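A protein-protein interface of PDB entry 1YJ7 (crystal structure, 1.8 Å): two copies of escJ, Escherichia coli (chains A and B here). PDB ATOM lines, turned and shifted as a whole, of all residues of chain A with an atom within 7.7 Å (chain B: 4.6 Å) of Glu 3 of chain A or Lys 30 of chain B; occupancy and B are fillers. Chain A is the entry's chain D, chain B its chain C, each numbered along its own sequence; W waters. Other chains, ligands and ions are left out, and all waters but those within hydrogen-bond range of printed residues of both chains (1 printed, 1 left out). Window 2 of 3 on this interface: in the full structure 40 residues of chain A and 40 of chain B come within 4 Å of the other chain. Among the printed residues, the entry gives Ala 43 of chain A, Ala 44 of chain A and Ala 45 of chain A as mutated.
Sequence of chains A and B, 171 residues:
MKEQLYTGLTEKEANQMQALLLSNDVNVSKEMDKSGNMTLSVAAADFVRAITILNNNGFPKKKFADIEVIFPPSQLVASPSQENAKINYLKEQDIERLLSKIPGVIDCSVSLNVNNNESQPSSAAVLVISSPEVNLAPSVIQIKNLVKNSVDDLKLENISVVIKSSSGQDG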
ATOM      1  N   LYS A   2      -4.891  27.364  12.214  1.00  0.00           N
ATOM      2  CA  LYS A   2      -5.001  26.830  13.612  1.00  0.00           C
ATOM      3  C   LYS A   2      -3.915  25.791  13.894  1.00  0.00           C
ATOM      4  O   LYS A   2      -3.623  24.934  13.061  1.00  0.00           O
ATOM      5  CB  LYS A   2      -6.383  26.208  13.865  1.00  0.00           C
ATOM      6  CG  LYS A   2      -7.527  27.223  14.070  1.00  0.00           C
ATOM      7  CD  LYS A   2      -7.400  28.037  15.379  1.00  0.00           C
ATOM      8  CE  LYS A   2      -8.761  28.394  15.996  1.00  0.00           C
ATOM      9  NZ  LYS A   2      -8.657  28.956  17.396  1.00  0.00           N
ATOM     10  N   GLU A   3      -3.323  25.891  15.081  1.00  0.00           N
ATOM     11  CA  GLU A   3      -2.309  24.980  15.564  1.00  0.00           C
ATOM     12  C   GLU A   3      -2.967  24.118  16.640  1.00  0.00           C
ATOM     13  O   GLU A   3      -3.601  24.641  17.551  1.00  0.00           O
ATOM     14  CB  GLU A   3      -1.167  25.796  16.163  1.00  0.00           C
ATOM     15  CG  GLU A   3       0.218  25.174  16.125  1.00  0.00           C
ATOM     16  CD  GLU A   3       0.691  24.800  14.733  1.00  0.00           C
ATOM     17  OE1 GLU A   3       0.767  23.597  14.486  1.00  0.00           O
ATOM     18  OE2 GLU A   3       0.985  25.695  13.900  1.00  0.00           O
ATOM     19  N   GLN A   4      -2.810  22.807  16.531  1.00  0.00           N
ATOM     20  CA  GLN A   4      -3.288  21.878  17.546  1.00  0.00           C
ATOM     21  C   GLN A   4      -2.443  21.971  18.807  1.00  0.00           C
ATOM     22  O   GLN A   4      -1.205  22.073  18.730  1.00  0.00           O
ATOM     23  CB  GLN A   4      -3.209  20.467  16.998  1.00  0.00           C
ATOM     24  CG  GLN A   4      -3.745  19.394  17.899  1.00  0.00           C
ATOM     25  CD  GLN A   4      -3.611  18.025  17.256  1.00  0.00           C
ATOM     26  OE1 GLN A   4      -2.660  17.287  17.547  1.00  0.00           O
ATOM     27  NE2 GLN A   4      -4.554  17.686  16.377  1.00  0.00           N
ATOM     28  N   LEU A   5      -3.114  21.956  19.962  1.00  0.00           N
ATOM     29  CA  LEU A   5      -2.438  21.867  21.256  1.00  0.00           C
ATOM     30  C   LEU A   5      -2.407  20.400  21.698  1.00  0.00           C
ATOM     31  O   LEU A   5      -1.341  19.772  21.718  1.00  0.00           O
ATOM     32  CB  LEU A   5      -3.137  22.745  22.310  1.00  0.00           C
ATOM     33  CG  LEU A   5      -3.049  24.250  22.102  1.00  0.00           C
ATOM     34  CD1 LEU A   5      -3.780  25.007  23.185  1.00  0.00           C
ATOM     35  CD2 LEU A   5      -1.624  24.719  21.996  1.00  0.00           C
ATOM     36  N   TYR A   6      -3.580  19.853  22.030  1.00  0.00           N
ATOM     37  CA  TYR A   6      -3.725  18.480  22.515  1.00  0.00           C
ATOM     38  C   TYR A   6      -5.019  17.853  22.031  1.00  0.00           C
ATOM     39  O   TYR A   6      -6.023  18.551  21.842  1.00  0.00           O
ATOM     40  CB  TYR A   6      -3.686  18.405  24.048  1.00  0.00           C
ATOM     41  CG  TYR A   6      -2.381  18.882  24.604  1.00  0.00           C
ATOM     42  CD1 TYR A   6      -2.227  20.166  25.108  1.00  0.00           C
ATOM     43  CD2 TYR A   6      -1.258  18.064  24.548  1.00  0.00           C
ATOM     44  CE1 TYR A   6      -0.994  20.608  25.588  1.00  0.00           C
ATOM     45  CE2 TYR A   6      -0.036  18.504  25.014  1.00  0.00           C
ATOM     46  CZ  TYR A   6       0.103  19.755  25.523  1.00  0.00           C
ATOM     47  OH  TYR A   6       1.360  20.146  25.965  1.00  0.00           O
ATOM     48  N   ASN A  27      -7.227  32.993  21.985  1.00  0.00           N
ATOM     49  CA  ASN A  27      -8.311  32.449  21.167  1.00  0.00           C
ATOM     50  C   ASN A  27      -8.139  30.929  21.043  1.00  0.00           C
ATOM     51  O   ASN A  27      -7.330  30.437  20.261  1.00  0.00           O
ATOM     52  CB  ASN A  27      -8.335  33.172  19.794  1.00  0.00           C
ATOM     53  CG  ASN A  27      -9.008  32.369  18.673  1.00  0.00           C
ATOM     54  OD1 ASN A  27      -9.860  31.505  18.908  1.00  0.00           O
ATOM     55  ND2 ASN A  27      -8.629  32.680  17.436  1.00  0.00           N
ATOM     56  N   SER A  29     -10.085  27.091  20.512  1.00  0.00           N
ATOM     57  CA  SER A  29     -11.246  26.372  20.035  1.00  0.00           C
ATOM     58  C   SER A  29     -11.166  24.920  20.468  1.00  0.00           C
ATOM     59  O   SER A  29     -10.084  24.338  20.573  1.00  0.00           O
ATOM     60  CB  SER A  29     -11.364  26.494  18.518  1.00  0.00           C
ATOM     61  OG  SER A  29     -10.234  25.948  17.888  1.00  0.00           O
ATOM     62  N   THR A  39     -10.285  17.962  21.765  1.00  0.00           N
ATOM     63  CA  THR A  39      -9.112  18.561  21.149  1.00  0.00           C
ATOM     64  C   THR A  39      -9.163  20.067  21.309  1.00  0.00           C
ATOM     65  O   THR A  39     -10.174  20.701  20.957  1.00  0.00           O
ATOM     66  CB  THR A  39      -9.096  18.243  19.639  1.00  0.00           C
ATOM     67  OG1 THR A  39      -8.921  16.840  19.451  1.00  0.00           O
ATOM     68  CG2 THR A  39      -7.905  18.905  18.941  1.00  0.00           C
ATOM     69  N   LEU A  40      -8.074  20.654  21.802  1.00  0.00           N
ATOM     70  CA  LEU A  40      -7.896  22.086  21.842  1.00  0.00           C
ATOM     71  C   LEU A  40      -6.914  22.555  20.786  1.00  0.00           C
ATOM     72  O   LEU A  40      -5.901  21.906  20.573  1.00  0.00           O
ATOM     73  CB  LEU A  40      -7.366  22.542  23.211  1.00  0.00           C
ATOM     74  CG  LEU A  40      -8.281  22.280  24.391  1.00  0.00           C
ATOM     75  CD1 LEU A  40      -7.603  22.742  25.676  1.00  0.00           C
ATOM     76  CD2 LEU A  40      -9.634  22.965  24.211  1.00  0.00           C
ATOM     77  N   SER A  41      -7.232  23.680  20.151  1.00  0.00           N
ATOM     78  CA  SER A  41      -6.385  24.345  19.159  1.00  0.00           C
ATOM     79  C   SER A  41      -6.393  25.844  19.374  1.00  0.00           C
ATOM     80  O   SER A  41      -7.278  26.390  20.016  1.00  0.00           O
ATOM     81  CB  SER A  41      -6.867  24.035  17.730  1.00  0.00           C
ATOM     82  OG  SER A  41      -7.124  22.657  17.569  1.00  0.00           O
ATOM     83  N   VAL A  42      -5.389  26.529  18.847  1.00  0.00           N
ATOM     84  CA  VAL A  42      -5.280  27.970  18.990  1.00  0.00           C
ATOM     85  C   VAL A  42      -4.800  28.553  17.677  1.00  0.00           C
ATOM     86  O   VAL A  42      -4.224  27.843  16.858  1.00  0.00           O
ATOM     87  CB  VAL A  42      -4.272  28.368  20.098  1.00  0.00           C
ATOM     88  CG1 VAL A  42      -4.805  27.982  21.460  1.00  0.00           C
ATOM     89  CG2 VAL A  42      -2.886  27.716  19.822  1.00  0.00           C
ATOM     90  N   ALA A  43      -5.033  29.845  17.484  1.00  0.00           N
ATOM     91  CA  ALA A  43      -4.447  30.583  16.363  1.00  0.00           C
ATOM     92  C   ALA A  43      -2.935  30.461  16.426  1.00  0.00           C
ATOM     93  O   ALA A  43      -2.363  30.507  17.520  1.00  0.00           O
ATOM     94  CB  ALA A  43      -4.853  32.048  16.430  1.00  0.00           C
ATOM     95  N   ALA A  44      -2.284  30.308  15.266  1.00  0.00           N
ATOM     96  CA  ALA A  44      -0.832  30.171  15.217  1.00  0.00           C
ATOM     97  C   ALA A  44      -0.106  31.310  15.921  1.00  0.00           C
ATOM     98  O   ALA A  44       0.931  31.100  16.535  1.00  0.00           O
ATOM     99  CB  ALA A  44      -0.336  30.059  13.749  1.00  0.00           C
ATOM    100  N   ALA A  45      -0.655  32.517  15.834  1.00  0.00           N
ATOM    101  CA  ALA A  45      -0.021  33.701  16.403  1.00  0.00           C
ATOM    102  C   ALA A  45      -0.062  33.676  17.934  1.00  0.00           C
ATOM    103  O   ALA A  45       0.686  34.394  18.595  1.00  0.00           O
ATOM    104  CB  ALA A  45      -0.692  34.962  15.870  1.00  0.00           C
ATOM    105  N   ASP A  46      -0.943  32.845  18.488  1.00  0.00           N
ATOM    106  CA  ASP A  46      -1.057  32.659  19.934  1.00  0.00           C
ATOM    107  C   ASP A  46      -0.405  31.362  20.446  1.00  0.00           C
ATOM    108  O   ASP A  46      -0.434  31.092  21.645  1.00  0.00           O
ATOM    109  CB  ASP A  46      -2.538  32.605  20.333  1.00  0.00           C
ATOM    110  CG  ASP A  46      -3.243  33.950  20.216  1.00  0.00           C
ATOM    111  OD1 ASP A  46      -2.591  35.016  20.306  1.00  0.00           O
ATOM    112  OD2 ASP A  46      -4.481  34.023  20.065  1.00  0.00           O
ATOM    113  N   PHE A  47       0.152  30.546  19.560  1.00  0.00           N
ATOM    114  CA  PHE A  47       0.687  29.245  19.976  1.00  0.00           C
ATOM    115  C   PHE A  47       1.749  29.328  21.066  1.00  0.00           C
ATOM    116  O   PHE A  47       1.676  28.603  22.076  1.00  0.00           O
ATOM    117  CB  PHE A  47       1.249  28.473  18.772  1.00  0.00           C
ATOM    118  CG  PHE A  47       1.736  27.109  19.128  1.00  0.00           C
ATOM    119  CD1 PHE A  47       0.861  26.058  19.257  1.00  0.00           C
ATOM    120  CD2 PHE A  47       3.076  26.893  19.405  1.00  0.00           C
ATOM    121  CE1 PHE A  47       1.315  24.781  19.596  1.00  0.00           C
ATOM    122  CE2 PHE A  47       3.527  25.649  19.748  1.00  0.00           C
ATOM    123  CZ  PHE A  47       2.652  24.589  19.848  1.00  0.00           C
ATOM    124  N   VAL A  48       2.754  30.183  20.880  1.00  0.00           N
ATOM    125  CA  VAL A  48       3.835  30.263  21.870  1.00  0.00           C
ATOM    126  C   VAL A  48       3.303  30.728  23.221  1.00  0.00           C
ATOM    127  O   VAL A  48       3.638  30.158  24.248  1.00  0.00           O
ATOM    128  CB  VAL A  48       4.993  31.175  21.402  1.00  0.00           C
ATOM    129  CG1 VAL A  48       5.992  31.412  22.524  1.00  0.00           C
ATOM    130  CG2 VAL A  48       5.675  30.552  20.188  1.00  0.00           C
ATOM    131  N   ILE A  51       1.319  27.816  24.919  1.00  0.00           N
ATOM    132  CA  ILE A  51       2.178  26.807  25.498  1.00  0.00           C
ATOM    133  C   ILE A  51       2.869  27.318  26.774  1.00  0.00           C
ATOM    134  O   ILE A  51       3.043  26.551  27.739  1.00  0.00           O
ATOM    135  CB  ILE A  51       3.187  26.320  24.421  1.00  0.00           C
ATOM    136  CG1 ILE A  51       2.427  25.576  23.311  1.00  0.00           C
ATOM    137  CG2 ILE A  51       4.250  25.405  25.038  1.00  0.00           C
ATOM    138  CD1 ILE A  51       1.581  24.408  23.762  1.00  0.00           C
ATOM    139  N   ALA B  14       6.424  17.630  21.306  1.00  0.00           N
ATOM    140  CA  ALA B  14       6.350  18.368  20.053  1.00  0.00           C
ATOM    141  C   ALA B  14       5.979  19.808  20.320  1.00  0.00           C
ATOM    142  O   ALA B  14       6.519  20.707  19.706  1.00  0.00           O
ATOM    143  CB  ALA B  14       5.363  17.732  19.082  1.00  0.00           C
ATOM    144  N   ASN B  15       5.051  20.047  21.244  1.00  0.00           N
ATOM    145  CA  ASN B  15       4.664  21.424  21.541  1.00  0.00           C
ATOM    146  C   ASN B  15       5.832  22.216  22.130  1.00  0.00           C
ATOM    147  O   ASN B  15       6.042  23.375  21.776  1.00  0.00           O
ATOM    148  CB  ASN B  15       3.485  21.489  22.512  1.00  0.00           C
ATOM    149  CG  ASN B  15       2.163  21.167  21.864  1.00  0.00           C
ATOM    150  OD1 ASN B  15       1.976  21.374  20.674  1.00  0.00           O
ATOM    151  ND2 ASN B  15       1.225  20.635  22.659  1.00  0.00           N
ATOM    152  N   GLN B  18       8.295  22.825  19.251  1.00  0.00           N
ATOM    153  CA  GLN B  18       7.719  23.811  18.343  1.00  0.00           C
ATOM    154  C   GLN B  18       7.772  25.227  18.917  1.00  0.00           C
ATOM    155  O   GLN B  18       8.208  26.157  18.248  1.00  0.00           O
ATOM    156  CB  GLN B  18       6.296  23.402  17.998  1.00  0.00           C
ATOM    157  CG  GLN B  18       5.554  24.360  17.064  1.00  0.00           C
ATOM    158  CD  GLN B  18       4.158  23.854  16.696  1.00  0.00           C
ATOM    159  OE1 GLN B  18       3.532  24.374  15.775  1.00  0.00           O
ATOM    160  NE2 GLN B  18       3.684  22.841  17.397  1.00  0.00           N
ATOM    161  N   VAL B  28       8.241  26.651  11.829  1.00  0.00           N
ATOM    162  CA  VAL B  28       8.150  25.213  11.994  1.00  0.00           C
ATOM    163  C   VAL B  28       6.701  24.810  11.781  1.00  0.00           C
ATOM    164  O   VAL B  28       5.785  25.554  12.126  1.00  0.00           O
ATOM    165  CB  VAL B  28       8.710  24.785  13.392  1.00  0.00           C
ATOM    166  CG1 VAL B  28       8.119  25.630  14.487  1.00  0.00           C
ATOM    167  CG2 VAL B  28       8.465  23.299  13.678  1.00  0.00           C
ATOM    168  N   SER B  29       6.497  23.667  11.149  1.00  0.00           N
ATOM    169  CA  SER B  29       5.169  23.123  10.941  1.00  0.00           C
ATOM    170  C   SER B  29       5.079  21.783  11.657  1.00  0.00           C
ATOM    171  O   SER B  29       6.089  21.092  11.838  1.00  0.00           O
ATOM    172  CB  SER B  29       4.865  22.976   9.445  1.00  0.00           C
ATOM    173  OG  SER B  29       5.573  21.897   8.862  1.00  0.00           O
ATOM    174  N   LYS B  30       3.863  21.433  12.054  1.00  0.00           N
ATOM    175  CA  LYS B  30       3.590  20.221  12.805  1.00  0.00           C
ATOM    176  C   LYS B  30       2.425  19.476  12.195  1.00  0.00           C
ATOM    177  O   LYS B  30       1.444  20.086  11.767  1.00  0.00           O
ATOM    178  CB  LYS B  30       3.252  20.590  14.255  1.00  0.00           C
ATOM    179  CG  LYS B  30       2.779  19.431  15.103  1.00  0.00           C
ATOM    180  CD  LYS B  30       2.688  19.838  16.584  1.00  0.00           C
ATOM    181  CE  LYS B  30       1.339  20.500  16.899  1.00  0.00           C
ATOM    182  NZ  LYS B  30       1.382  21.217  18.210  1.00  0.00           N
ATOM    183  N   GLU B  31       2.525  18.155  12.166  1.00  0.00           N
ATOM    184  CA  GLU B  31       1.415  17.323  11.727  1.00  0.00           C
ATOM    185  C   GLU B  31       1.362  16.027  12.523  1.00  0.00           C
ATOM    186  O   GLU B  31       2.353  15.629  13.146  1.00  0.00           O
ATOM    187  CB  GLU B  31       1.493  17.080  10.209  1.00  0.00           C
ATOM    188  CG  GLU B  31       2.529  16.063   9.773  1.00  0.00           C
ATOM    189  CD  GLU B  31       2.846  16.092   8.284  1.00  0.00           C
ATOM    190  OE1 GLU B  31       3.707  15.283   7.865  1.00  0.00           O
ATOM    191  OE2 GLU B  31       2.262  16.908   7.537  1.00  0.00           O
ATOM    192  N   MET B  38       3.519  12.899  16.671  1.00  0.00           N
ATOM    193  CA  MET B  38       3.720  14.196  16.047  1.00  0.00           C
ATOM    194  C   MET B  38       5.051  14.274  15.286  1.00  0.00           C
ATOM    195  O   MET B  38       6.076  13.773  15.746  1.00  0.00           O
ATOM    196  CB  MET B  38       3.657  15.299  17.098  1.00  0.00           C
ATOM    197  CG  MET B  38       2.412  15.227  17.990  1.00  0.00           C
ATOM    198  SD  MET B  38       0.834  15.188  17.065  1.00  0.00           S
ATOM    199  CE  MET B  38       0.909  16.645  16.233  1.00  0.00           C
ATOM    200  N   THR B  39       4.990  14.942  14.141  1.00  0.00           N
ATOM    201  CA  THR B  39       6.129  15.247  13.295  1.00  0.00           C
ATOM    202  C   THR B  39       6.353  16.744  13.222  1.00  0.00           C
ATOM    203  O   THR B  39       5.404  17.505  13.002  1.00  0.00           O
ATOM    204  CB  THR B  39       5.853  14.702  11.878  1.00  0.00           C
ATOM    205  OG1 THR B  39       5.838  13.274  11.919  1.00  0.00           O
ATOM    206  CG2 THR B  39       6.965  15.063  10.914  1.00  0.00           C
ATOM    207  N   LEU B  40       7.595  17.188  13.393  1.00  0.00           N
ATOM    208  CA  LEU B  40       7.963  18.588  13.213  1.00  0.00           C
ATOM    209  C   LEU B  40       8.862  18.731  11.986  1.00  0.00           C
ATOM    210  O   LEU B  40       9.735  17.892  11.773  1.00  0.00           O
ATOM    211  CB  LEU B  40       8.729  19.127  14.422  1.00  0.00           C
ATOM    212  CG  LEU B  40       7.933  19.290  15.718  1.00  0.00           C
ATOM    213  CD1 LEU B  40       8.807  19.864  16.819  1.00  0.00           C
ATOM    214  CD2 LEU B  40       6.738  20.199  15.482  1.00  0.00           C
HETATM  215  O   HOH W   1       1.778  23.557  11.560  1.00  0.00           O
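Positions printed for both chains: 29, 39 and 40. Of the 11 pairs that touch across the chains among the printed residues, none has its exchanged pair printed and touching as well.
The side-chain amide nitrogen (NE2) of Gln 18 of chain B sits close to the side-chain amino group (NZ) of Lys 30 of chain B (2.9 Å). O of Tyr 6 of chain A is in hydrogen-bond range of N of Leu 40 of chain A (2.9 Å). The backbone carbonyl oxygen (O) of Leu 40 of chain A sits at hydrogen-bond distance from the backbone NH (N) of Leu 5 of chain A (2.9 Å). The backbone NH (N) of Glu 3 of chain A is in hydrogen-bond range of the backbone carbonyl oxygen (O) of Val 42 of chain A (2.8 Å). The side-chain amide oxygen of Asn 15 of chain B is in hydrogen-bond range of the side-chain amino group of Lys 30 of chain B (2.5 Å).
Of chain B, only Gln 18 (3.1 Å) and Lys 30 (3.9 Å) come within 4 Å of Glu 3 of chain A. Printed residues of chain B within 4 Å of Gln 4 of chain A: Asn 15, Lys 30 and Met 38. Printed residues of chain B within 4 Å of Leu 5 of chain A: Asn 15 (2.9 Å). Ser 29 of chain A touches none of the printed residues of chain B. Printed residues of chain B within 4 Å of Phe 47 of chain A: Asn 15, Gln 18 and Lys 30. Printed residues of chain B within 4 Å of Ile 51 of chain A: Asn 15 (3.7 Å). Of the printed residues of chain A, Gln 18 of chain B touches Glu 3 (3.1 Å) and Phe 47 (3.2 Å). The nearest residue of chain A that does not touch Lys 30 of chain B is Leu 5 of chain A (4.7 Å). The nearest printed residue of chain A that does not touch Gln 18 of chain B is Gln 4 of chain A (5.1 Å).
Printed residues of chain A that touch a printed residue of chain B: Glu 3, Gln 4, Leu 5, Tyr 6, Phe 47 and Ile 51. Hydrophobic or aromatic side chains of chain A within 4 Å of the printed part of chain B: Tyr 6, Phe 47 and Ile 51. Among the printed residues, 11 pairs touch across the chains. Among the printed residues, no Asp or Glu carboxylate lies within 4 Å of a Lys or Arg side-chain nitrogen of the other chain.
OH of Tyr 6 of chain A lies close to ND2 of Asn 15 of chain B (3.3 Å). O of Gln 4 of chain A is in hydrogen-bond range of NZ of Lys 30 of chain B (2.8 Å). ND2 of Asn 15 of chain B lies within hydrogen-bond range of O of Leu 5 of chain A (2.9 Å). OE1 of Gln 18 of chain B lies close to OE1 of Glu 3 of chain A (3.1 Å).
Water W1 lies within hydrogen-bond range of N of Lys 30 of chain B and OE1 of Glu 3 of chain A.
Among the printed residues, pairs that only touch across the chains: Phe 47 of chain A with Gln 18 of chain B (3.2 Å), Phe 47 of chain A with Asn 15 of chain B (3.4 Å), Ile 51 of chain A with Asn 15 of chain B (3.7 Å), Gln 4 of chain A with Asn 15 of chain B (3.8 Å), Phe 47 of chain A with Lys 30 of chain B (3.8 Å), Gln 4 of chain A with Met 38 of chain B (3.9 Å) and Glu 3 of chain A with Lys 30 of chain B (3.9 Å).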
